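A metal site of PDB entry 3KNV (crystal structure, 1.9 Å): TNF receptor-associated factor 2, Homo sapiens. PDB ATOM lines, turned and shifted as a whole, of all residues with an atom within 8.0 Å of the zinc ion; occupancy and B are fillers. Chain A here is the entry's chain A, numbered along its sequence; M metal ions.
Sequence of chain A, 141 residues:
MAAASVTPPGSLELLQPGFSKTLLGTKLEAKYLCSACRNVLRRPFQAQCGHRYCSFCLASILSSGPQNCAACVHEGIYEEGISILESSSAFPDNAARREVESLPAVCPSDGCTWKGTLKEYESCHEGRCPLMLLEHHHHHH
SG of Cys 37 lies close to N of Gly 18 (3.5 Å).
The backbone NH of Cys 34 is in hydrogen-bond range of the backbone carbonyl oxygen of Asn 39 (2.8 Å).
The side-chain amide oxygen of Gln 16 lies close to the backbone carbonyl oxygen of Cys 37, 2.7 Å away.
The side-chain sulfur (SG) of Cys 54 sits close to the backbone NH (N) of Arg 42, at 3.4 Å.
The side-chain sulfur (SG) of Cys 34 lies close to the backbone NH (N) of Ala 36 (3.2 Å).
The backbone NH (N) of Asn 39 lies close to the side-chain sulfur (SG) of Cys 37, 3.4 Å away.
The guanidinium group (NH1) of Arg 38 is in hydrogen-bond range of the backbone carbonyl oxygen (O) of Cys 34 (2.9 Å).
The nearest printed residue that does not touch the zinc ion is Gly 18 (4.02 Å).
The zinc ion is bound by SG of Cys 57 (2.2 Å), SG of Cys 54 (2.4 Å), SG of Cys 37 (2.5 Å) and SG of Cys 34 (2.5 Å).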
ATOM      1  N   LEU A  15      25.630 -35.492 -27.113  1.00  0.00           N
ATOM      2  CA  LEU A  15      25.194 -34.935 -25.799  1.00  0.00           C
ATOM      3  C   LEU A  15      26.131 -33.812 -25.356  1.00  0.00           C
ATOM      4  O   LEU A  15      26.231 -33.502 -24.175  1.00  0.00           O
ATOM      5  CB  LEU A  15      25.165 -36.045 -24.741  1.00  0.00           C
ATOM      6  CG  LEU A  15      24.619 -35.688 -23.346  1.00  0.00           C
ATOM      7  CD1 LEU A  15      23.183 -35.211 -23.461  1.00  0.00           C
ATOM      8  CD2 LEU A  15      24.710 -36.910 -22.446  1.00  0.00           C
ATOM      9  N   GLN A  16      26.807 -33.207 -26.328  1.00  0.00           N
ATOM     10  CA  GLN A  16      27.743 -32.115 -26.067  1.00  0.00           C
ATOM     11  C   GLN A  16      27.203 -30.816 -26.649  1.00  0.00           C
ATOM     12  O   GLN A  16      27.418 -30.521 -27.822  1.00  0.00           O
ATOM     13  CB  GLN A  16      29.105 -32.424 -26.698  1.00  0.00           C
ATOM     14  CG  GLN A  16      29.736 -33.708 -26.214  1.00  0.00           C
ATOM     15  CD  GLN A  16      30.017 -33.684 -24.726  1.00  0.00           C
ATOM     16  OE1 GLN A  16      30.793 -32.871 -24.238  1.00  0.00           O
ATOM     17  NE2 GLN A  16      29.362 -34.583 -23.991  1.00  0.00           N
ATOM     18  N   PRO A  17      26.476 -30.029 -25.834  1.00  0.00           N
ATOM     19  CA  PRO A  17      25.910 -28.757 -26.312  1.00  0.00           C
ATOM     20  C   PRO A  17      26.974 -27.763 -26.753  1.00  0.00           C
ATOM     21  O   PRO A  17      26.809 -27.068 -27.758  1.00  0.00           O
ATOM     22  CB  PRO A  17      25.129 -28.262 -25.100  1.00  0.00           C
ATOM     23  CG  PRO A  17      24.745 -29.526 -24.383  1.00  0.00           C
ATOM     24  CD  PRO A  17      26.031 -30.318 -24.459  1.00  0.00           C
ATOM     25  N   GLY A  18      28.062 -27.683 -26.006  1.00  0.00           N
ATOM     26  CA  GLY A  18      29.130 -26.762 -26.346  1.00  0.00           C
ATOM     27  C   GLY A  18      29.778 -27.028 -27.687  1.00  0.00           C
ATOM     28  O   GLY A  18      29.618 -28.100 -28.268  1.00  0.00           O
ATOM     29  N   PHE A  19      30.523 -26.044 -28.189  1.00  0.00           N
ATOM     30  CA  PHE A  19      31.204 -26.158 -29.464  1.00  0.00           C
ATOM     31  C   PHE A  19      32.398 -27.106 -29.366  1.00  0.00           C
ATOM     32  O   PHE A  19      33.147 -27.069 -28.393  1.00  0.00           O
ATOM     33  CB  PHE A  19      31.716 -24.782 -29.920  1.00  0.00           C
ATOM     34  CG  PHE A  19      30.634 -23.772 -30.166  1.00  0.00           C
ATOM     35  CD1 PHE A  19      29.834 -23.860 -31.308  1.00  0.00           C
ATOM     36  CD2 PHE A  19      30.397 -22.753 -29.252  1.00  0.00           C
ATOM     37  CE1 PHE A  19      28.827 -22.932 -31.536  1.00  0.00           C
ATOM     38  CE2 PHE A  19      29.384 -21.818 -29.483  1.00  0.00           C
ATOM     39  CZ  PHE A  19      28.598 -21.910 -30.628  1.00  0.00           C
ATOM     40  N   LEU A  33      36.205 -23.255 -21.654  1.00  0.00           N
ATOM     41  CA  LEU A  33      35.427 -24.489 -21.580  1.00  0.00           C
ATOM     42  C   LEU A  33      34.310 -24.509 -20.554  1.00  0.00           C
ATOM     43  O   LEU A  33      34.419 -23.958 -19.455  1.00  0.00           O
ATOM     44  CB  LEU A  33      36.362 -25.677 -21.322  1.00  0.00           C
ATOM     45  CG  LEU A  33      37.507 -25.892 -22.318  1.00  0.00           C
ATOM     46  CD1 LEU A  33      38.305 -27.114 -21.896  1.00  0.00           C
ATOM     47  CD2 LEU A  33      36.957 -26.068 -23.729  1.00  0.00           C
ATOM     48  N   CYS A  34      33.220 -25.160 -20.945  1.00  0.00           N
ATOM     49  CA  CYS A  34      32.051 -25.317 -20.099  1.00  0.00           C
ATOM     50  C   CYS A  34      32.396 -26.233 -18.937  1.00  0.00           C
ATOM     51  O   CYS A  34      33.063 -27.269 -19.125  1.00  0.00           O
ATOM     52  CB  CYS A  34      30.904 -25.924 -20.916  1.00  0.00           C
ATOM     53  SG  CYS A  34      29.414 -26.317 -19.968  1.00  0.00           S
ATOM     54  N   SER A  35      31.946 -25.866 -17.750  1.00  0.00           N
ATOM     55  CA  SER A  35      32.202 -26.659 -16.552  1.00  0.00           C
ATOM     56  C   SER A  35      31.462 -27.992 -16.580  1.00  0.00           C
ATOM     57  O   SER A  35      31.760 -28.904 -15.803  1.00  0.00           O
ATOM     58  CB  SER A  35      31.787 -25.876 -15.313  1.00  0.00           C
ATOM     59  OG  SER A  35      32.509 -24.663 -15.217  1.00  0.00           O
ATOM     60  N   ALA A  36      30.498 -28.120 -17.498  1.00  0.00           N
ATOM     61  CA  ALA A  36      29.713 -29.334 -17.604  1.00  0.00           C
ATOM     62  C   ALA A  36      30.090 -30.259 -18.762  1.00  0.00           C
ATOM     63  O   ALA A  36      30.518 -31.402 -18.535  1.00  0.00           O
ATOM     64  CB  ALA A  36      28.233 -28.986 -17.688  1.00  0.00           C
ATOM     65  N   CYS A  37      29.931 -29.797 -19.992  1.00  0.00           N
ATOM     66  CA  CYS A  37      30.224 -30.631 -21.157  1.00  0.00           C
ATOM     67  C   CYS A  37      31.691 -30.618 -21.566  1.00  0.00           C
ATOM     68  O   CYS A  37      32.109 -31.408 -22.411  1.00  0.00           O
ATOM     69  CB  CYS A  37      29.360 -30.219 -22.342  1.00  0.00           C
ATOM     70  SG  CYS A  37      29.829 -28.656 -23.086  1.00  0.00           S
ATOM     71  N   ARG A  38      32.467 -29.706 -20.979  1.00  0.00           N
ATOM     72  CA  ARG A  38      33.886 -29.595 -21.267  1.00  0.00           C
ATOM     73  C   ARG A  38      34.207 -29.185 -22.698  1.00  0.00           C
ATOM     74  O   ARG A  38      35.346 -29.316 -23.148  1.00  0.00           O
ATOM     75  CB  ARG A  38      34.597 -30.912 -20.932  1.00  0.00           C
ATOM     76  CG  ARG A  38      34.306 -31.402 -19.519  1.00  0.00           C
ATOM     77  CD  ARG A  38      34.560 -30.296 -18.496  1.00  0.00           C
ATOM     78  NE  ARG A  38      35.973 -29.949 -18.408  1.00  0.00           N
ATOM     79  CZ  ARG A  38      36.421 -28.734 -18.100  1.00  0.00           C
ATOM     80  NH1 ARG A  38      35.567 -27.749 -17.850  1.00  0.00           N
ATOM     81  NH2 ARG A  38      37.733 -28.509 -18.014  1.00  0.00           N
ATOM     82  N   ASN A  39      33.205 -28.697 -23.420  1.00  0.00           N
ATOM     83  CA  ASN A  39      33.418 -28.220 -24.786  1.00  0.00           C
ATOM     84  C   ASN A  39      33.474 -26.699 -24.700  1.00  0.00           C
ATOM     85  O   ASN A  39      33.352 -26.123 -23.622  1.00  0.00           O
ATOM     86  CB  ASN A  39      32.271 -28.672 -25.707  1.00  0.00           C
ATOM     87  CG  ASN A  39      32.568 -29.988 -26.399  1.00  0.00           C
ATOM     88  OD1 ASN A  39      33.467 -30.732 -25.997  1.00  0.00           O
ATOM     89  ND2 ASN A  39      31.801 -30.291 -27.446  1.00  0.00           N
ATOM     90  N   VAL A  40      33.680 -26.022 -25.826  1.00  0.00           N
ATOM     91  CA  VAL A  40      33.747 -24.562 -25.806  1.00  0.00           C
ATOM     92  C   VAL A  40      32.390 -23.971 -25.456  1.00  0.00           C
ATOM     93  O   VAL A  40      31.364 -24.358 -26.002  1.00  0.00           O
ATOM     94  CB  VAL A  40      34.210 -24.020 -27.165  1.00  0.00           C
ATOM     95  CG1 VAL A  40      34.292 -22.492 -27.111  1.00  0.00           C
ATOM     96  CG2 VAL A  40      35.575 -24.608 -27.521  1.00  0.00           C
ATOM     97  N   LEU A  41      32.388 -23.014 -24.520  1.00  0.00           N
ATOM     98  CA  LEU A  41      31.169 -22.347 -24.064  1.00  0.00           C
ATOM     99  C   LEU A  41      30.261 -21.814 -25.176  1.00  0.00           C
ATOM    100  O   LEU A  41      30.697 -21.047 -26.029  1.00  0.00           O
ATOM    101  CB  LEU A  41      31.540 -21.193 -23.138  1.00  0.00           C
ATOM    102  CG  LEU A  41      32.134 -21.528 -21.764  1.00  0.00           C
ATOM    103  CD1 LEU A  41      32.765 -20.294 -21.142  1.00  0.00           C
ATOM    104  CD2 LEU A  41      31.031 -22.088 -20.875  1.00  0.00           C
ATOM    105  N   ARG A  42      28.989 -22.223 -25.140  1.00  0.00           N
ATOM    106  CA  ARG A  42      27.989 -21.763 -26.104  1.00  0.00           C
ATOM    107  C   ARG A  42      26.963 -20.949 -25.308  1.00  0.00           C
ATOM    108  O   ARG A  42      26.223 -21.513 -24.492  1.00  0.00           O
ATOM    109  CB  ARG A  42      27.297 -22.962 -26.781  1.00  0.00           C
ATOM    110  CG  ARG A  42      26.196 -22.567 -27.768  1.00  0.00           C
ATOM    111  CD  ARG A  42      25.333 -23.762 -28.173  1.00  0.00           C
ATOM    112  NE  ARG A  42      26.058 -24.773 -28.937  1.00  0.00           N
ATOM    113  CZ  ARG A  42      26.284 -24.726 -30.254  1.00  0.00           C
ATOM    114  NH1 ARG A  42      25.838 -23.700 -30.973  1.00  0.00           N
ATOM    115  NH2 ARG A  42      26.947 -25.707 -30.848  1.00  0.00           N
ATOM    116  N   ARG A  52      31.548 -21.165 -15.275  1.00  0.00           N
ATOM    117  CA  ARG A  52      30.736 -20.925 -16.451  1.00  0.00           C
ATOM    118  C   ARG A  52      30.181 -22.206 -17.070  1.00  0.00           C
ATOM    119  O   ARG A  52      30.831 -23.257 -17.055  1.00  0.00           O
ATOM    120  CB  ARG A  52      31.548 -20.164 -17.494  1.00  0.00           C
ATOM    121  CG  ARG A  52      32.191 -18.890 -16.953  1.00  0.00           C
ATOM    122  CD  ARG A  52      32.943 -18.161 -18.051  1.00  0.00           C
ATOM    123  NE  ARG A  52      33.473 -16.873 -17.607  1.00  0.00           N
ATOM    124  CZ  ARG A  52      34.662 -16.691 -17.050  1.00  0.00           C
ATOM    125  NH1 ARG A  52      35.477 -17.719 -16.856  1.00  0.00           N
ATOM    126  NH2 ARG A  52      35.044 -15.469 -16.702  1.00  0.00           N
ATOM    127  N   TYR A  53      28.970 -22.098 -17.609  1.00  0.00           N
ATOM    128  CA  TYR A  53      28.288 -23.227 -18.239  1.00  0.00           C
ATOM    129  C   TYR A  53      27.571 -22.760 -19.498  1.00  0.00           C
ATOM    130  O   TYR A  53      27.124 -21.613 -19.566  1.00  0.00           O
ATOM    131  CB  TYR A  53      27.213 -23.792 -17.318  1.00  0.00           C
ATOM    132  CG  TYR A  53      27.711 -24.442 -16.051  1.00  0.00           C
ATOM    133  CD1 TYR A  53      28.139 -23.672 -14.969  1.00  0.00           C
ATOM    134  CD2 TYR A  53      27.725 -25.829 -15.936  1.00  0.00           C
ATOM    135  CE1 TYR A  53      28.579 -24.286 -13.787  1.00  0.00           C
ATOM    136  CE2 TYR A  53      28.160 -26.444 -14.779  1.00  0.00           C
ATOM    137  CZ  TYR A  53      28.579 -25.674 -13.707  1.00  0.00           C
ATOM    138  OH  TYR A  53      29.012 -26.308 -12.560  1.00  0.00           O
ATOM    139  N   CYS A  54      27.455 -23.658 -20.483  1.00  0.00           N
ATOM    140  CA  CYS A  54      26.716 -23.336 -21.693  1.00  0.00           C
ATOM    141  C   CYS A  54      25.280 -23.130 -21.219  1.00  0.00           C
ATOM    142  O   CYS A  54      24.835 -23.796 -20.279  1.00  0.00           O
ATOM    143  CB  CYS A  54      26.704 -24.514 -22.674  1.00  0.00           C
ATOM    144  SG  CYS A  54      28.292 -24.979 -23.324  1.00  0.00           S
ATOM    145  N   SER A  55      24.551 -22.227 -21.864  1.00  0.00           N
ATOM    146  CA  SER A  55      23.176 -21.981 -21.495  1.00  0.00           C
ATOM    147  C   SER A  55      22.383 -23.302 -21.466  1.00  0.00           C
ATOM    148  O   SER A  55      21.644 -23.575 -20.520  1.00  0.00           O
ATOM    149  CB  SER A  55      22.528 -21.020 -22.506  1.00  0.00           C
ATOM    150  OG  SER A  55      21.203 -20.726 -22.118  1.00  0.00           O
ATOM    151  N   PHE A  56      22.557 -24.107 -22.514  1.00  0.00           N
ATOM    152  CA  PHE A  56      21.865 -25.390 -22.607  1.00  0.00           C
ATOM    153  C   PHE A  56      22.262 -26.352 -21.488  1.00  0.00           C
ATOM    154  O   PHE A  56      21.402 -27.022 -20.902  1.00  0.00           O
ATOM    155  CB  PHE A  56      22.167 -26.057 -23.959  1.00  0.00           C
ATOM    156  CG  PHE A  56      21.457 -25.421 -25.126  1.00  0.00           C
ATOM    157  CD1 PHE A  56      21.975 -25.518 -26.408  1.00  0.00           C
ATOM    158  CD2 PHE A  56      20.244 -24.751 -24.941  1.00  0.00           C
ATOM    159  CE1 PHE A  56      21.294 -24.958 -27.497  1.00  0.00           C
ATOM    160  CE2 PHE A  56      19.555 -24.195 -26.024  1.00  0.00           C
ATOM    161  CZ  PHE A  56      20.093 -24.303 -27.304  1.00  0.00           C
ATOM    162  N   CYS A  57      23.543 -26.403 -21.183  1.00  0.00           N
ATOM    163  CA  CYS A  57      24.048 -27.287 -20.140  1.00  0.00           C
ATOM    164  C   CYS A  57      23.523 -26.920 -18.763  1.00  0.00           C
ATOM    165  O   CYS A  57      23.132 -27.807 -17.983  1.00  0.00           O
ATOM    166  CB  CYS A  57      25.567 -27.267 -20.121  1.00  0.00           C
ATOM    167  SG  CYS A  57      26.272 -27.954 -21.621  1.00  0.00           S
ATOM    168  N   LEU A  58      23.515 -25.626 -18.441  1.00  0.00           N
ATOM    169  CA  LEU A  58      23.045 -25.183 -17.141  1.00  0.00           C
ATOM    170  C   LEU A  58      21.553 -25.431 -16.995  1.00  0.00           C
ATOM    171  O   LEU A  58      21.097 -25.878 -15.941  1.00  0.00           O
ATOM    172  CB  LEU A  58      23.343 -23.688 -16.940  1.00  0.00           C
ATOM    173  CG  LEU A  58      22.943 -23.127 -15.563  1.00  0.00           C
ATOM    174  CD1 LEU A  58      23.738 -23.854 -14.471  1.00  0.00           C
ATOM    175  CD2 LEU A  58      23.203 -21.635 -15.508  1.00  0.00           C
ATOM    176  N   ILE A  61      20.975 -29.134 -16.264  1.00  0.00           N
ATOM    177  CA  ILE A  61      21.357 -29.404 -14.884  1.00  0.00           C
ATOM    178  C   ILE A  61      20.312 -28.899 -13.902  1.00  0.00           C
ATOM    179  O   ILE A  61      20.001 -29.576 -12.920  1.00  0.00           O
ATOM    180  CB  ILE A  61      22.717 -28.727 -14.547  1.00  0.00           C
ATOM    181  CG1 ILE A  61      23.844 -29.411 -15.321  1.00  0.00           C
ATOM    182  CG2 ILE A  61      22.972 -28.785 -13.049  1.00  0.00           C
ATOM    183  CD1 ILE A  61      25.196 -28.748 -15.149  1.00  0.00           C
HETATM  184 ZN    ZN M   1      28.275 -27.046 -22.038  1.00  0.00          ZN
